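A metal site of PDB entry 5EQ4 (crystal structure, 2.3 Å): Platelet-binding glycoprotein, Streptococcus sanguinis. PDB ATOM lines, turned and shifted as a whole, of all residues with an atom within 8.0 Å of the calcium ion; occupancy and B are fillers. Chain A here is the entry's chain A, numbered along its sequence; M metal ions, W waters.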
ATOM      1  N   ALA A 122       6.370   5.579  -1.484  1.00  0.00           N
ATOM      2  CA  ALA A 122       6.902   4.585  -0.566  1.00  0.00           C
ATOM      3  C   ALA A 122       8.279   5.008  -0.075  1.00  0.00           C
ATOM      4  O   ALA A 122       9.013   5.740  -0.757  1.00  0.00           O
ATOM      5  CB  ALA A 122       6.987   3.213  -1.237  1.00  0.00           C
ATOM      6  N   GLN A 123       8.638   4.547   1.129  1.00  0.00           N
ATOM      7  CA  GLN A 123       9.872   5.012   1.748  1.00  0.00           C
ATOM      8  C   GLN A 123      11.111   4.549   0.994  1.00  0.00           C
ATOM      9  O   GLN A 123      12.135   5.249   1.012  1.00  0.00           O
ATOM     10  CB  GLN A 123       9.934   4.557   3.207  1.00  0.00           C
ATOM     11  CG  GLN A 123       8.986   5.319   4.127  1.00  0.00           C
ATOM     12  CD  GLN A 123       9.116   4.902   5.575  1.00  0.00           C
ATOM     13  OE1 GLN A 123       8.578   3.875   5.986  1.00  0.00           O
ATOM     14  NE2 GLN A 123       9.819   5.707   6.363  1.00  0.00           N
ATOM     15  N   THR A 124      11.050   3.400   0.317  1.00  0.00           N
ATOM     16  CA  THR A 124      12.212   2.934  -0.426  1.00  0.00           C
ATOM     17  C   THR A 124      12.554   3.827  -1.605  1.00  0.00           C
ATOM     18  O   THR A 124      13.684   3.790  -2.084  1.00  0.00           O
ATOM     19  CB  THR A 124      12.004   1.492  -0.913  1.00  0.00           C
ATOM     20  OG1 THR A 124      13.218   1.016  -1.514  1.00  0.00           O
ATOM     21  CG2 THR A 124      10.884   1.431  -1.945  1.00  0.00           C
ATOM     22  N   ASP A 125      11.590   4.623  -2.087  1.00  0.00           N
ATOM     23  CA  ASP A 125      11.904   5.611  -3.116  1.00  0.00           C
ATOM     24  C   ASP A 125      12.851   6.686  -2.585  1.00  0.00           C
ATOM     25  O   ASP A 125      13.603   7.276  -3.357  1.00  0.00           O
ATOM     26  CB  ASP A 125      10.620   6.256  -3.641  1.00  0.00           C
ATOM     27  CG  ASP A 125       9.717   5.271  -4.342  1.00  0.00           C
ATOM     28  OD1 ASP A 125       9.939   4.056  -4.209  1.00  0.00           O
ATOM     29  OD2 ASP A 125       8.775   5.729  -5.031  1.00  0.00           O
ATOM     30  N   LYS A 126      12.825   6.923  -1.274  1.00  0.00           N
ATOM     31  CA  LYS A 126      13.657   7.979  -0.702  1.00  0.00           C
ATOM     32  C   LYS A 126      15.052   7.475  -0.356  1.00  0.00           C
ATOM     33  O   LYS A 126      16.032   8.221  -0.476  1.00  0.00           O
ATOM     34  CB  LYS A 126      12.963   8.557   0.541  1.00  0.00           C
ATOM     35  CG  LYS A 126      13.794   9.556   1.333  1.00  0.00           C
ATOM     36  CD  LYS A 126      13.063   9.976   2.598  1.00  0.00           C
ATOM     37  CE  LYS A 126      13.915  10.900   3.458  1.00  0.00           C
ATOM     38  NZ  LYS A 126      13.223  11.304   4.712  1.00  0.00           N
ATOM     39  N   TYR A 127      15.171   6.217   0.058  1.00  0.00           N
ATOM     40  CA  TYR A 127      16.404   5.689   0.623  1.00  0.00           C
ATOM     41  C   TYR A 127      17.107   4.759  -0.360  1.00  0.00           C
ATOM     42  O   TYR A 127      16.471   3.877  -0.941  1.00  0.00           O
ATOM     43  CB  TYR A 127      16.130   4.962   1.936  1.00  0.00           C
ATOM     44  CG  TYR A 127      15.472   5.822   2.983  1.00  0.00           C
ATOM     45  CD1 TYR A 127      16.164   6.846   3.612  1.00  0.00           C
ATOM     46  CD2 TYR A 127      14.144   5.619   3.342  1.00  0.00           C
ATOM     47  CE1 TYR A 127      15.572   7.642   4.563  1.00  0.00           C
ATOM     48  CE2 TYR A 127      13.527   6.411   4.298  1.00  0.00           C
ATOM     49  CZ  TYR A 127      14.247   7.420   4.907  1.00  0.00           C
ATOM     50  OH  TYR A 127      13.643   8.208   5.860  1.00  0.00           O
ATOM     51  N   ASN A 128      18.398   4.979  -0.541  1.00  0.00           N
ATOM     52  CA  ASN A 128      19.282   4.072  -1.281  1.00  0.00           C
ATOM     53  C   ASN A 128      20.370   3.608  -0.322  1.00  0.00           C
ATOM     54  O   ASN A 128      21.275   4.403   0.000  1.00  0.00           O
ATOM     55  CB  ASN A 128      19.886   4.762  -2.495  1.00  0.00           C
ATOM     56  CG  ASN A 128      18.861   5.514  -3.322  1.00  0.00           C
ATOM     57  OD1 ASN A 128      18.167   4.924  -4.141  1.00  0.00           O
ATOM     58  ND2 ASN A 128      18.766   6.816  -3.107  1.00  0.00           N
ATOM     59  N   PRO A 129      20.318   2.375   0.177  1.00  0.00           N
ATOM     60  CA  PRO A 129      21.231   1.981   1.258  1.00  0.00           C
ATOM     61  C   PRO A 129      22.678   1.862   0.785  1.00  0.00           C
ATOM     62  O   PRO A 129      22.953   1.404  -0.328  1.00  0.00           O
ATOM     63  CB  PRO A 129      20.685   0.636   1.716  1.00  0.00           C
ATOM     64  CG  PRO A 129      19.974   0.091   0.518  1.00  0.00           C
ATOM     65  CD  PRO A 129      19.412   1.281  -0.210  1.00  0.00           C
ATOM     66  N   ILE A 178      16.172  -4.909   3.759  1.00  0.00           N
ATOM     67  CA  ILE A 178      15.854  -3.717   4.541  1.00  0.00           C
ATOM     68  C   ILE A 178      14.375  -3.428   4.352  1.00  0.00           C
ATOM     69  O   ILE A 178      13.970  -2.932   3.294  1.00  0.00           O
ATOM     70  CB  ILE A 178      16.714  -2.513   4.141  1.00  0.00           C
ATOM     71  CG1 ILE A 178      18.200  -2.799   4.407  1.00  0.00           C
ATOM     72  CG2 ILE A 178      16.274  -1.262   4.882  1.00  0.00           C
ATOM     73  CD1 ILE A 178      19.107  -1.631   4.081  1.00  0.00           C
ATOM     74  N   TYR A 180      11.450  -1.180   5.315  1.00  0.00           N
ATOM     75  CA  TYR A 180      11.167   0.121   5.895  1.00  0.00           C
ATOM     76  C   TYR A 180       9.845   0.081   6.676  1.00  0.00           C
ATOM     77  O   TYR A 180       9.068  -0.861   6.544  1.00  0.00           O
ATOM     78  CB  TYR A 180      11.137   1.183   4.806  1.00  0.00           C
ATOM     79  CG  TYR A 180      12.456   1.307   4.086  1.00  0.00           C
ATOM     80  CD1 TYR A 180      13.529   1.975   4.680  1.00  0.00           C
ATOM     81  CD2 TYR A 180      12.648   0.748   2.828  1.00  0.00           C
ATOM     82  CE1 TYR A 180      14.745   2.091   4.029  1.00  0.00           C
ATOM     83  CE2 TYR A 180      13.865   0.850   2.176  1.00  0.00           C
ATOM     84  CZ  TYR A 180      14.907   1.527   2.785  1.00  0.00           C
ATOM     85  OH  TYR A 180      16.122   1.634   2.145  1.00  0.00           O
ATOM     86  N   SER A 184       7.832  -1.289   2.571  1.00  0.00           N
ATOM     87  CA  SER A 184       8.632  -1.306   1.352  1.00  0.00           C
ATOM     88  C   SER A 184      10.035  -1.789   1.669  1.00  0.00           C
ATOM     89  O   SER A 184      10.498  -1.731   2.815  1.00  0.00           O
ATOM     90  CB  SER A 184       8.667   0.079   0.711  1.00  0.00           C
ATOM     91  OG  SER A 184       9.271   1.034   1.573  1.00  0.00           O
ATOM     92  N   THR A 185      10.734  -2.281   0.646  1.00  0.00           N
ATOM     93  CA  THR A 185      11.977  -3.003   0.865  1.00  0.00           C
ATOM     94  C   THR A 185      13.087  -2.514  -0.062  1.00  0.00           C
ATOM     95  O   THR A 185      12.835  -1.989  -1.150  1.00  0.00           O
ATOM     96  CB  THR A 185      11.799  -4.521   0.647  1.00  0.00           C
ATOM     97  OG1 THR A 185      11.393  -4.777  -0.705  1.00  0.00           O
ATOM     98  CG2 THR A 185      10.739  -5.081   1.601  1.00  0.00           C
ATOM     99  N   ASP A 186      14.314  -2.689   0.410  1.00  0.00           N
ATOM    100  CA  ASP A 186      15.517  -2.641  -0.408  1.00  0.00           C
ATOM    101  C   ASP A 186      16.304  -3.919  -0.174  1.00  0.00           C
ATOM    102  O   ASP A 186      16.145  -4.586   0.846  1.00  0.00           O
ATOM    103  CB  ASP A 186      16.384  -1.412  -0.077  1.00  0.00           C
ATOM    104  CG  ASP A 186      15.938  -0.152  -0.804  1.00  0.00           C
ATOM    105  OD1 ASP A 186      15.560  -0.244  -1.991  1.00  0.00           O
ATOM    106  OD2 ASP A 186      15.972   0.932  -0.183  1.00  0.00           O
ATOM    107  N   THR A 187      17.163  -4.260  -1.135  1.00  0.00           N
ATOM    108  CA  THR A 187      17.924  -5.498  -1.080  1.00  0.00           C
ATOM    109  C   THR A 187      19.392  -5.237  -1.391  1.00  0.00           C
ATOM    110  O   THR A 187      19.718  -4.506  -2.339  1.00  0.00           O
ATOM    111  CB  THR A 187      17.361  -6.536  -2.064  1.00  0.00           C
ATOM    112  OG1 THR A 187      15.970  -6.762  -1.783  1.00  0.00           O
ATOM    113  CG2 THR A 187      18.115  -7.858  -1.941  1.00  0.00           C
HETATM  114 CA    CA M   1      15.335   2.130  -2.071  1.00  0.00          CA
HETATM  115  O   HOH W   1      18.108   1.501  -3.479  1.00  0.00           O
HETATM  116  O   HOH W   2      14.431   1.683  -4.388  1.00  0.00           O
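The side-chain carboxylate (OD2) of Asp 186 lies close to the side-chain hydroxyl (OH) of Tyr 180 (2.4 Å). OG of Ser 184 is in hydrogen-bond range of N of Thr 124. The side-chain hydroxyl of Thr 124 sits close to the backbone carbonyl oxygen of Thr 185 (3.1 Å). N of Asp 186 is in hydrogen-bond range of O of Ile 178. OH of Tyr 127 sits at hydrogen-bond distance from NZ of Lys 126, at 3.3 Å.
The nearest printed residue that does not touch the calcium ion is Tyr 180 (4.3 Å).
The calcium ion is bound by the side-chain carboxylate (OD2) of Asp 186, the backbone carbonyl oxygen (O) of Thr 124, the backbone carbonyl oxygen (O) of Tyr 127, the side-chain carboxylate (OD1) of Asp 186, the side-chain hydroxyl (OG1) of Thr 124 and water W2.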
